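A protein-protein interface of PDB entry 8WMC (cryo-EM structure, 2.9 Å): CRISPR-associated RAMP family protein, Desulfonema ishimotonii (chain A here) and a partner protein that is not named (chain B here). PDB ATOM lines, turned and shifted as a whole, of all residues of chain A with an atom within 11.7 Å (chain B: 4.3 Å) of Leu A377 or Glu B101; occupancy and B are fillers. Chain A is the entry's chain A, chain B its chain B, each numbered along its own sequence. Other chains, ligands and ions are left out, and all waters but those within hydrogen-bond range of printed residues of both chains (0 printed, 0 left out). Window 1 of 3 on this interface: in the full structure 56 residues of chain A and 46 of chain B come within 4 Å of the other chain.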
ATOM      1  N   VAL A 172     -13.872 -36.473  15.861  1.00  0.00           N
ATOM      2  CA  VAL A 172     -12.684 -35.670  15.585  1.00  0.00           C
ATOM      3  C   VAL A 172     -11.451 -36.509  15.881  1.00  0.00           C
ATOM      4  O   VAL A 172     -11.421 -37.266  16.860  1.00  0.00           O
ATOM      5  CB  VAL A 172     -12.689 -34.373  16.418  1.00  0.00           C
ATOM      6  CG1 VAL A 172     -11.336 -33.679  16.350  1.00  0.00           C
ATOM      7  CG2 VAL A 172     -13.789 -33.437  15.945  1.00  0.00           C
ATOM      8  N   LYS A 182       0.984 -31.182  22.602  1.00  0.00           N
ATOM      9  CA  LYS A 182      -0.296 -30.558  22.309  1.00  0.00           C
ATOM     10  C   LYS A 182      -0.620 -30.742  20.833  1.00  0.00           C
ATOM     11  O   LYS A 182       0.276 -30.797  19.988  1.00  0.00           O
ATOM     12  CB  LYS A 182      -0.280 -29.060  22.661  1.00  0.00           C
ATOM     13  CG  LYS A 182      -1.635 -28.377  22.556  1.00  0.00           C
ATOM     14  CD  LYS A 182      -1.555 -26.908  22.920  1.00  0.00           C
ATOM     15  CE  LYS A 182      -2.892 -26.221  22.697  1.00  0.00           C
ATOM     16  NZ  LYS A 182      -2.816 -24.754  22.920  1.00  0.00           N
ATOM     17  N   ALA A 183      -1.913 -30.839  20.534  1.00  0.00           N
ATOM     18  CA  ALA A 183      -2.386 -30.987  19.166  1.00  0.00           C
ATOM     19  C   ALA A 183      -2.693 -29.623  18.564  1.00  0.00           C
ATOM     20  O   ALA A 183      -3.230 -28.742  19.240  1.00  0.00           O
ATOM     21  CB  ALA A 183      -3.633 -31.868  19.117  1.00  0.00           C
ATOM     22  N   HIS A 184      -2.352 -29.463  17.281  1.00  0.00           N
ATOM     23  CA  HIS A 184      -2.528 -28.207  16.563  1.00  0.00           C
ATOM     24  C   HIS A 184      -3.457 -28.305  15.360  1.00  0.00           C
ATOM     25  O   HIS A 184      -3.828 -27.264  14.810  1.00  0.00           O
ATOM     26  CB  HIS A 184      -1.166 -27.673  16.093  1.00  0.00           C
ATOM     27  CG  HIS A 184      -0.252 -27.288  17.213  1.00  0.00           C
ATOM     28  ND1 HIS A 184       0.883 -28.005  17.529  1.00  0.00           N
ATOM     29  CD2 HIS A 184      -0.305 -26.263  18.095  1.00  0.00           C
ATOM     30  CE1 HIS A 184       1.489 -27.436  18.556  1.00  0.00           C
ATOM     31  NE2 HIS A 184       0.788 -26.377  18.919  1.00  0.00           N
ATOM     32  N   ASP A 185      -3.841 -29.508  14.937  1.00  0.00           N
ATOM     33  CA  ASP A 185      -4.745 -29.673  13.808  1.00  0.00           C
ATOM     34  C   ASP A 185      -5.463 -31.005  13.949  1.00  0.00           C
ATOM     35  O   ASP A 185      -5.064 -31.866  14.736  1.00  0.00           O
ATOM     36  CB  ASP A 185      -3.997 -29.602  12.473  1.00  0.00           C
ATOM     37  CG  ASP A 185      -2.735 -30.432  12.474  1.00  0.00           C
ATOM     38  OD1 ASP A 185      -2.358 -30.930  13.553  1.00  0.00           O
ATOM     39  OD2 ASP A 185      -2.120 -30.586  11.399  1.00  0.00           O
ATOM     40  N   PHE A 186      -6.537 -31.165  13.182  1.00  0.00           N
ATOM     41  CA  PHE A 186      -7.325 -32.390  13.230  1.00  0.00           C
ATOM     42  C   PHE A 186      -8.097 -32.537  11.926  1.00  0.00           C
ATOM     43  O   PHE A 186      -7.979 -31.720  11.009  1.00  0.00           O
ATOM     44  CB  PHE A 186      -8.262 -32.396  14.444  1.00  0.00           C
ATOM     45  CG  PHE A 186      -9.320 -31.323  14.416  1.00  0.00           C
ATOM     46  CD1 PHE A 186     -10.539 -31.534  13.791  1.00  0.00           C
ATOM     47  CD2 PHE A 186      -9.104 -30.111  15.040  1.00  0.00           C
ATOM     48  CE1 PHE A 186     -11.505 -30.553  13.774  1.00  0.00           C
ATOM     49  CE2 PHE A 186     -10.071 -29.133  15.030  1.00  0.00           C
ATOM     50  CZ  PHE A 186     -11.271 -29.352  14.394  1.00  0.00           C
ATOM     51  N   LYS A 371     -21.078 -12.821  29.249  1.00  0.00           N
ATOM     52  CA  LYS A 371     -21.173 -14.269  29.086  1.00  0.00           C
ATOM     53  C   LYS A 371     -19.878 -14.764  28.451  1.00  0.00           C
ATOM     54  O   LYS A 371     -19.654 -14.583  27.251  1.00  0.00           O
ATOM     55  CB  LYS A 371     -22.389 -14.634  28.242  1.00  0.00           C
ATOM     56  CG  LYS A 371     -23.713 -14.338  28.929  1.00  0.00           C
ATOM     57  CD  LYS A 371     -24.898 -14.740  28.069  1.00  0.00           C
ATOM     58  CE  LYS A 371     -26.214 -14.418  28.758  1.00  0.00           C
ATOM     59  NZ  LYS A 371     -27.390 -14.793  27.928  1.00  0.00           N
ATOM     60  N   ILE A 372     -19.031 -15.394  29.264  1.00  0.00           N
ATOM     61  CA  ILE A 372     -17.751 -15.902  28.786  1.00  0.00           C
ATOM     62  C   ILE A 372     -17.938 -17.295  28.190  1.00  0.00           C
ATOM     63  O   ILE A 372     -18.880 -18.021  28.516  1.00  0.00           O
ATOM     64  CB  ILE A 372     -16.715 -15.911  29.926  1.00  0.00           C
ATOM     65  CG1 ILE A 372     -15.291 -16.006  29.373  1.00  0.00           C
ATOM     66  CG2 ILE A 372     -16.991 -17.053  30.903  1.00  0.00           C
ATOM     67  CD1 ILE A 372     -14.221 -15.774  30.419  1.00  0.00           C
ATOM     68  N   THR A 373     -17.025 -17.663  27.291  1.00  0.00           N
ATOM     69  CA  THR A 373     -17.015 -18.977  26.654  1.00  0.00           C
ATOM     70  C   THR A 373     -15.607 -19.544  26.742  1.00  0.00           C
ATOM     71  O   THR A 373     -14.653 -18.915  26.273  1.00  0.00           O
ATOM     72  CB  THR A 373     -17.468 -18.891  25.193  1.00  0.00           C
ATOM     73  OG1 THR A 373     -16.640 -17.959  24.485  1.00  0.00           O
ATOM     74  CG2 THR A 373     -18.919 -18.442  25.109  1.00  0.00           C
ATOM     75  N   ARG A 374     -15.479 -20.734  27.332  1.00  0.00           N
ATOM     76  CA  ARG A 374     -14.175 -21.350  27.536  1.00  0.00           C
ATOM     77  C   ARG A 374     -13.727 -22.211  26.361  1.00  0.00           C
ATOM     78  O   ARG A 374     -12.519 -22.332  26.128  1.00  0.00           O
ATOM     79  CB  ARG A 374     -14.178 -22.198  28.817  1.00  0.00           C
ATOM     80  CG  ARG A 374     -15.228 -23.310  28.867  1.00  0.00           C
ATOM     81  CD  ARG A 374     -15.071 -24.178  30.111  1.00  0.00           C
ATOM     82  NE  ARG A 374     -13.798 -24.890  30.137  1.00  0.00           N
ATOM     83  CZ  ARG A 374     -13.515 -25.971  29.418  1.00  0.00           C
ATOM     84  NH1 ARG A 374     -14.395 -26.503  28.582  1.00  0.00           N
ATOM     85  NH2 ARG A 374     -12.315 -26.532  29.538  1.00  0.00           N
ATOM     86  N   ARG A 375     -14.661 -22.804  25.621  1.00  0.00           N
ATOM     87  CA  ARG A 375     -14.340 -23.603  24.439  1.00  0.00           C
ATOM     88  C   ARG A 375     -14.252 -22.651  23.253  1.00  0.00           C
ATOM     89  O   ARG A 375     -15.272 -22.227  22.705  1.00  0.00           O
ATOM     90  CB  ARG A 375     -15.391 -24.685  24.218  1.00  0.00           C
ATOM     91  CG  ARG A 375     -14.981 -25.767  23.232  1.00  0.00           C
ATOM     92  CD  ARG A 375     -16.169 -26.253  22.415  1.00  0.00           C
ATOM     93  NE  ARG A 375     -17.249 -26.753  23.259  1.00  0.00           N
ATOM     94  CZ  ARG A 375     -18.455 -27.098  22.825  1.00  0.00           C
ATOM     95  NH1 ARG A 375     -18.787 -27.012  21.546  1.00  0.00           N
ATOM     96  NH2 ARG A 375     -19.355 -27.541  23.699  1.00  0.00           N
ATOM     97  N   ILE A 376     -13.026 -22.312  22.852  1.00  0.00           N
ATOM     98  CA  ILE A 376     -12.806 -21.280  21.846  1.00  0.00           C
ATOM     99  C   ILE A 376     -11.461 -21.512  21.174  1.00  0.00           C
ATOM    100  O   ILE A 376     -10.507 -21.984  21.799  1.00  0.00           O
ATOM    101  CB  ILE A 376     -12.868 -19.868  22.474  1.00  0.00           C
ATOM    102  CG1 ILE A 376     -12.926 -18.801  21.383  1.00  0.00           C
ATOM    103  CG2 ILE A 376     -11.667 -19.627  23.387  1.00  0.00           C
ATOM    104  CD1 ILE A 376     -13.117 -17.418  21.915  1.00  0.00           C
ATOM    105  N   LEU A 377     -11.393 -21.156  19.891  1.00  0.00           N
ATOM    106  CA  LEU A 377     -10.163 -21.187  19.098  1.00  0.00           C
ATOM    107  C   LEU A 377      -9.527 -22.577  19.120  1.00  0.00           C
ATOM    108  O   LEU A 377      -8.408 -22.780  19.598  1.00  0.00           O
ATOM    109  CB  LEU A 377      -9.179 -20.115  19.577  1.00  0.00           C
ATOM    110  CG  LEU A 377      -9.505 -18.681  19.146  1.00  0.00           C
ATOM    111  CD1 LEU A 377      -8.714 -17.688  19.976  1.00  0.00           C
ATOM    112  CD2 LEU A 377      -9.229 -18.468  17.662  1.00  0.00           C
ATOM    113  N   GLY A 378     -10.280 -23.539  18.594  1.00  0.00           N
ATOM    114  CA  GLY A 378      -9.822 -24.907  18.443  1.00  0.00           C
ATOM    115  C   GLY A 378      -9.930 -25.411  17.018  1.00  0.00           C
ATOM    116  O   GLY A 378      -9.285 -26.399  16.660  1.00  0.00           O
ATOM    117  N   ASP A 379     -10.736 -24.741  16.193  1.00  0.00           N
ATOM    118  CA  ASP A 379     -10.934 -25.159  14.809  1.00  0.00           C
ATOM    119  C   ASP A 379      -9.631 -25.002  14.037  1.00  0.00           C
ATOM    120  O   ASP A 379      -9.191 -23.881  13.763  1.00  0.00           O
ATOM    121  CB  ASP A 379     -12.053 -24.345  14.169  1.00  0.00           C
ATOM    122  CG  ASP A 379     -13.428 -24.814  14.594  1.00  0.00           C
ATOM    123  OD1 ASP A 379     -13.567 -25.276  15.746  1.00  0.00           O
ATOM    124  OD2 ASP A 379     -14.369 -24.723  13.778  1.00  0.00           O
ATOM    125  N   ALA A 380      -9.009 -26.129  13.705  1.00  0.00           N
ATOM    126  CA  ALA A 380      -7.764 -26.183  12.949  1.00  0.00           C
ATOM    127  C   ALA A 380      -7.815 -27.325  11.944  1.00  0.00           C
ATOM    128  O   ALA A 380      -6.861 -28.099  11.810  1.00  0.00           O
ATOM    129  CB  ALA A 380      -6.565 -26.334  13.880  1.00  0.00           C
ATOM    130  N   GLU A 381      -8.937 -27.455  11.238  1.00  0.00           N
ATOM    131  CA  GLU A 381      -9.131 -28.577  10.328  1.00  0.00           C
ATOM    132  C   GLU A 381      -8.097 -28.555   9.210  1.00  0.00           C
ATOM    133  O   GLU A 381      -7.789 -27.503   8.644  1.00  0.00           O
ATOM    134  CB  GLU A 381     -10.542 -28.542   9.742  1.00  0.00           C
ATOM    135  CG  GLU A 381     -10.854 -29.714   8.825  1.00  0.00           C
ATOM    136  CD  GLU A 381     -12.318 -30.112   8.842  1.00  0.00           C
ATOM    137  OE1 GLU A 381     -13.170 -29.269   9.193  1.00  0.00           O
ATOM    138  OE2 GLU A 381     -12.618 -31.276   8.503  1.00  0.00           O
ATOM    139  N   THR A 702       0.539 -14.081  35.093  1.00  0.00           N
ATOM    140  CA  THR A 702      -0.578 -14.601  34.311  1.00  0.00           C
ATOM    141  C   THR A 702      -0.331 -16.036  33.861  1.00  0.00           C
ATOM    142  O   THR A 702      -1.286 -16.807  33.707  1.00  0.00           O
ATOM    143  CB  THR A 702      -0.825 -13.703  33.099  1.00  0.00           C
ATOM    144  OG1 THR A 702      -1.136 -12.376  33.542  1.00  0.00           O
ATOM    145  CG2 THR A 702      -1.977 -14.234  32.258  1.00  0.00           C
ATOM    146  N   HIS A 703       0.929 -16.405  33.626  1.00  0.00           N
ATOM    147  CA  HIS A 703       1.361 -17.734  33.196  1.00  0.00           C
ATOM    148  C   HIS A 703       0.838 -18.121  31.816  1.00  0.00           C
ATOM    149  O   HIS A 703       0.929 -19.296  31.437  1.00  0.00           O
ATOM    150  CB  HIS A 703       0.969 -18.817  34.213  1.00  0.00           C
ATOM    151  CG  HIS A 703       1.715 -18.724  35.508  1.00  0.00           C
ATOM    152  ND1 HIS A 703       3.092 -18.734  35.576  1.00  0.00           N
ATOM    153  CD2 HIS A 703       1.275 -18.618  36.783  1.00  0.00           C
ATOM    154  CE1 HIS A 703       3.466 -18.639  36.840  1.00  0.00           C
ATOM    155  NE2 HIS A 703       2.382 -18.567  37.592  1.00  0.00           N
ATOM    156  N   SER A 704       0.308 -17.171  31.045  1.00  0.00           N
ATOM    157  CA  SER A 704      -0.071 -17.412  29.658  1.00  0.00           C
ATOM    158  C   SER A 704       1.119 -17.071  28.772  1.00  0.00           C
ATOM    159  O   SER A 704       1.549 -15.913  28.724  1.00  0.00           O
ATOM    160  CB  SER A 704      -1.292 -16.577  29.273  1.00  0.00           C
ATOM    161  OG  SER A 704      -2.387 -16.850  30.130  1.00  0.00           O
ATOM    162  N   ASP A 705       1.650 -18.076  28.075  1.00  0.00           N
ATOM    163  CA  ASP A 705       2.874 -17.928  27.292  1.00  0.00           C
ATOM    164  C   ASP A 705       4.036 -17.519  28.201  1.00  0.00           C
ATOM    165  O   ASP A 705       4.656 -16.466  28.039  1.00  0.00           O
ATOM    166  CB  ASP A 705       2.672 -16.923  26.152  1.00  0.00           C
ATOM    167  CG  ASP A 705       3.715 -17.060  25.063  1.00  0.00           C
ATOM    168  OD1 ASP A 705       3.692 -18.079  24.342  1.00  0.00           O
ATOM    169  OD2 ASP A 705       4.556 -16.147  24.925  1.00  0.00           O
ATOM    170  N   GLU A 717      -0.512 -24.006  29.117  1.00  0.00           N
ATOM    171  CA  GLU A 717      -1.398 -24.177  27.971  1.00  0.00           C
ATOM    172  C   GLU A 717      -0.632 -24.551  26.709  1.00  0.00           C
ATOM    173  O   GLU A 717      -1.192 -25.227  25.840  1.00  0.00           O
ATOM    174  CB  GLU A 717      -2.197 -22.889  27.741  1.00  0.00           C
ATOM    175  CG  GLU A 717      -3.209 -22.934  26.595  1.00  0.00           C
ATOM    176  CD  GLU A 717      -4.332 -23.921  26.846  1.00  0.00           C
ATOM    177  OE1 GLU A 717      -4.623 -24.201  28.028  1.00  0.00           O
ATOM    178  OE2 GLU A 717      -4.930 -24.410  25.865  1.00  0.00           O
ATOM    179  N   TYR A 718       0.624 -24.127  26.590  1.00  0.00           N
ATOM    180  CA  TYR A 718       1.448 -24.393  25.419  1.00  0.00           C
ATOM    181  C   TYR A 718       2.390 -25.579  25.597  1.00  0.00           C
ATOM    182  O   TYR A 718       3.170 -25.866  24.685  1.00  0.00           O
ATOM    183  CB  TYR A 718       2.261 -23.144  25.070  1.00  0.00           C
ATOM    184  CG  TYR A 718       1.417 -21.991  24.579  1.00  0.00           C
ATOM    185  CD1 TYR A 718       1.044 -21.896  23.247  1.00  0.00           C
ATOM    186  CD2 TYR A 718       0.991 -20.998  25.450  1.00  0.00           C
ATOM    187  CE1 TYR A 718       0.274 -20.845  22.795  1.00  0.00           C
ATOM    188  CE2 TYR A 718       0.221 -19.943  25.007  1.00  0.00           C
ATOM    189  CZ  TYR A 718      -0.136 -19.871  23.679  1.00  0.00           C
ATOM    190  OH  TYR A 718      -0.904 -18.824  23.229  1.00  0.00           O
ATOM    191  N   ARG B  97      -0.945 -10.490  22.108  1.00  0.00           N
ATOM    192  CA  ARG B  97      -1.604 -11.766  21.864  1.00  0.00           C
ATOM    193  C   ARG B  97      -2.591 -12.098  22.976  1.00  0.00           C
ATOM    194  O   ARG B  97      -3.738 -12.472  22.707  1.00  0.00           O
ATOM    195  CB  ARG B  97      -0.542 -12.859  21.727  1.00  0.00           C
ATOM    196  CG  ARG B  97      -1.068 -14.259  21.442  1.00  0.00           C
ATOM    197  CD  ARG B  97       0.076 -15.257  21.332  1.00  0.00           C
ATOM    198  NE  ARG B  97       0.952 -14.951  20.199  1.00  0.00           N
ATOM    199  CZ  ARG B  97       2.270 -14.770  20.240  1.00  0.00           C
ATOM    200  NH1 ARG B  97       2.963 -14.865  21.366  1.00  0.00           N
ATOM    201  NH2 ARG B  97       2.915 -14.486  19.114  1.00  0.00           N
ATOM    202  N   GLU B  98      -2.165 -11.967  24.235  1.00  0.00           N
ATOM    203  CA  GLU B  98      -3.062 -12.308  25.338  1.00  0.00           C
ATOM    204  C   GLU B  98      -4.251 -11.354  25.393  1.00  0.00           C
ATOM    205  O   GLU B  98      -5.388 -11.776  25.657  1.00  0.00           O
ATOM    206  CB  GLU B  98      -2.303 -12.319  26.666  1.00  0.00           C
ATOM    207  CG  GLU B  98      -1.737 -10.982  27.103  1.00  0.00           C
ATOM    208  CD  GLU B  98      -0.894 -11.088  28.361  1.00  0.00           C
ATOM    209  OE1 GLU B  98      -0.731 -12.212  28.878  1.00  0.00           O
ATOM    210  OE2 GLU B  98      -0.396 -10.044  28.834  1.00  0.00           O
ATOM    211  N   THR B  99      -4.018 -10.063  25.129  1.00  0.00           N
ATOM    212  CA  THR B  99      -5.127  -9.118  25.105  1.00  0.00           C
ATOM    213  C   THR B  99      -6.115  -9.454  23.991  1.00  0.00           C
ATOM    214  O   THR B  99      -7.333  -9.361  24.184  1.00  0.00           O
ATOM    215  CB  THR B  99      -4.592  -7.696  24.946  1.00  0.00           C
ATOM    216  OG1 THR B  99      -3.536  -7.472  25.888  1.00  0.00           O
ATOM    217  CG2 THR B  99      -5.695  -6.676  25.176  1.00  0.00           C
ATOM    218  N   LEU B 100      -5.611  -9.849  22.818  1.00  0.00           N
ATOM    219  CA  LEU B 100      -6.505 -10.223  21.726  1.00  0.00           C
ATOM    220  C   LEU B 100      -7.305 -11.475  22.066  1.00  0.00           C
ATOM    221  O   LEU B 100      -8.492 -11.572  21.726  1.00  0.00           O
ATOM    222  CB  LEU B 100      -5.706 -10.428  20.440  1.00  0.00           C
ATOM    223  CG  LEU B 100      -5.369  -9.132  19.701  1.00  0.00           C
ATOM    224  CD1 LEU B 100      -4.130  -9.305  18.847  1.00  0.00           C
ATOM    225  CD2 LEU B 100      -6.546  -8.671  18.857  1.00  0.00           C
ATOM    226  N   GLU B 101      -6.671 -12.451  22.724  1.00  0.00           N
ATOM    227  CA  GLU B 101      -7.405 -13.626  23.193  1.00  0.00           C
ATOM    228  C   GLU B 101      -8.541 -13.229  24.124  1.00  0.00           C
ATOM    229  O   GLU B 101      -9.675 -13.706  23.979  1.00  0.00           O
ATOM    230  CB  GLU B 101      -6.460 -14.600  23.901  1.00  0.00           C
ATOM    231  CG  GLU B 101      -5.418 -15.255  23.013  1.00  0.00           C
ATOM    232  CD  GLU B 101      -6.035 -16.194  21.998  1.00  0.00           C
ATOM    233  OE1 GLU B 101      -7.079 -16.803  22.309  1.00  0.00           O
ATOM    234  OE2 GLU B 101      -5.475 -16.332  20.893  1.00  0.00           O
ATOM    235  N   GLN B 102      -8.256 -12.349  25.087  1.00  0.00           N
ATOM    236  CA  GLN B 102      -9.299 -11.907  26.009  1.00  0.00           C
ATOM    237  C   GLN B 102     -10.431 -11.206  25.267  1.00  0.00           C
ATOM    238  O   GLN B 102     -11.615 -11.454  25.538  1.00  0.00           O
ATOM    239  CB  GLN B 102      -8.701 -10.980  27.066  1.00  0.00           C
ATOM    240  CG  GLN B 102      -8.049 -11.705  28.229  1.00  0.00           C
ATOM    241  CD  GLN B 102      -7.442 -10.753  29.239  1.00  0.00           C
ATOM    242  OE1 GLN B 102      -7.952  -9.654  29.457  1.00  0.00           O
ATOM    243  NE2 GLN B 102      -6.347 -11.172  29.862  1.00  0.00           N
ATOM    244  N   ILE B 103     -10.083 -10.337  24.314  1.00  0.00           N
ATOM    245  CA  ILE B 103     -11.095  -9.575  23.585  1.00  0.00           C
ATOM    246  C   ILE B 103     -11.996 -10.515  22.789  1.00  0.00           C
ATOM    247  O   ILE B 103     -13.227 -10.390  22.810  1.00  0.00           O
ATOM    248  CB  ILE B 103     -10.419  -8.528  22.677  1.00  0.00           C
ATOM    249  CG1 ILE B 103      -9.753  -7.431  23.512  1.00  0.00           C
ATOM    250  CG2 ILE B 103     -11.425  -7.894  21.738  1.00  0.00           C
ATOM    251  CD1 ILE B 103      -8.606  -6.741  22.804  1.00  0.00           C
ATOM    252  N   ILE B 104     -11.394 -11.476  22.084  1.00  0.00           N
ATOM    253  CA  ILE B 104     -12.174 -12.407  21.269  1.00  0.00           C
ATOM    254  C   ILE B 104     -13.074 -13.260  22.156  1.00  0.00           C
ATOM    255  O   ILE B 104     -14.252 -13.495  21.844  1.00  0.00           O
ATOM    256  CB  ILE B 104     -11.237 -13.282  20.412  1.00  0.00           C
ATOM    257  CG1 ILE B 104     -10.528 -12.445  19.343  1.00  0.00           C
ATOM    258  CG2 ILE B 104     -12.011 -14.404  19.742  1.00  0.00           C
ATOM    259  CD1 ILE B 104      -9.208 -13.033  18.894  1.00  0.00           C
ATOM    260  N   ARG B 105     -12.526 -13.743  23.277  1.00  0.00           N
ATOM    261  CA  ARG B 105     -13.298 -14.596  24.172  1.00  0.00           C
ATOM    262  C   ARG B 105     -14.490 -13.848  24.748  1.00  0.00           C
ATOM    263  O   ARG B 105     -15.572 -14.428  24.895  1.00  0.00           O
ATOM    264  CB  ARG B 105     -12.385 -15.132  25.282  1.00  0.00           C
ATOM    265  CG  ARG B 105     -13.072 -15.921  26.399  1.00  0.00           C
ATOM    266  CD  ARG B 105     -12.086 -16.312  27.488  1.00  0.00           C
ATOM    267  NE  ARG B 105     -11.020 -17.174  26.975  1.00  0.00           N
ATOM    268  CZ  ARG B 105      -9.714 -16.920  26.999  1.00  0.00           C
ATOM    269  NH1 ARG B 105      -9.219 -15.800  27.509  1.00  0.00           N
ATOM    270  NH2 ARG B 105      -8.875 -17.820  26.495  1.00  0.00           N
ATOM    271  N   TYR B 128     -10.106 -10.990  15.106  1.00  0.00           N
ATOM    272  CA  TYR B 128      -9.776 -12.274  14.492  1.00  0.00           C
ATOM    273  C   TYR B 128      -8.657 -12.124  13.472  1.00  0.00           C
ATOM    274  O   TYR B 128      -7.746 -12.957  13.416  1.00  0.00           O
ATOM    275  CB  TYR B 128     -11.010 -12.884  13.826  1.00  0.00           C
ATOM    276  CG  TYR B 128     -11.793 -13.838  14.699  1.00  0.00           C
ATOM    277  CD1 TYR B 128     -11.254 -15.056  15.088  1.00  0.00           C
ATOM    278  CD2 TYR B 128     -13.078 -13.528  15.119  1.00  0.00           C
ATOM    279  CE1 TYR B 128     -11.965 -15.930  15.881  1.00  0.00           C
ATOM    280  CE2 TYR B 128     -13.799 -14.397  15.910  1.00  0.00           C
ATOM    281  CZ  TYR B 128     -13.239 -15.597  16.287  1.00  0.00           C
ATOM    282  OH  TYR B 128     -13.954 -16.468  17.077  1.00  0.00           O
ATOM    283  N   ARG B 131      -5.333 -11.579  15.357  1.00  0.00           N
ATOM    284  CA  ARG B 131      -4.877 -12.806  16.000  1.00  0.00           C
ATOM    285  C   ARG B 131      -4.371 -13.806  14.969  1.00  0.00           C
ATOM    286  O   ARG B 131      -3.378 -14.503  15.207  1.00  0.00           O
ATOM    287  CB  ARG B 131      -6.003 -13.412  16.842  1.00  0.00           C
ATOM    288  CG  ARG B 131      -5.633 -14.689  17.617  1.00  0.00           C
ATOM    289  CD  ARG B 131      -4.618 -14.443  18.730  1.00  0.00           C
ATOM    290  NE  ARG B 131      -3.960 -15.679  19.149  1.00  0.00           N
ATOM    291  CZ  ARG B 131      -2.778 -16.110  18.722  1.00  0.00           C
ATOM    292  NH1 ARG B 131      -2.079 -15.457  17.806  1.00  0.00           N
ATOM    293  NH2 ARG B 131      -2.285 -17.239  19.222  1.00  0.00           N
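Of the printed residues of chain B, Ile A372 touches Arg B105.
Of the printed residues of chain B, Thr A373 touches Arg B105.
Of the printed residues of chain B, Ile A376 touches Ile B104 (3.9 Å) and Arg B105 (3.6 Å).
Of chain B, only Glu B101 comes within 4 Å of Leu A377.
Gly A378 touches none of the printed residues of chain B.
Glu B98 touches none of the printed residues of chain A.
Glu B101 touches just one residue of chain A: Leu A377 (3.0 Å).
No residue of chain A comes within 4 Å of Gln B102.
No residue of chain A comes within 4 Å of Ile B103.
Ile B104 touches one residue of chain A.
Of chain A, only Ile A372, Thr A373 and Ile A376 come within 4 Å of Arg B105.
No residue of chain A comes within 4 Å of Arg B131.
The nearest residue of chain B that does not touch Leu A377 is Tyr B128 (4.1 Å).
The nearest printed residue of chain B that does not touch Ile A376 is Tyr B128 (5.0 Å).
CD1 of Ile A372 touches CD of Arg B105 (3.7 Å).
Thr A373 touches Arg B105 (O to CG, 3.4 Å).
Ile B104 touches Ile A376 (CG2 to CD1, 3.9 Å).
Arg B105 touches Ile A376.
Leu A377 touches Glu B101.
The side-chain carboxylate (OE2) of Glu B101 lies within salt-bridge range of the guanidinium group (NE) of Arg B131, at 2.4 Å.
Of the 11 printed residues of chain B, 3 touch a printed residue of chain A.
Printed residues of chain A that touch a printed residue of chain B: Ile A372, Thr A373, Ile A376 and Leu A377.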
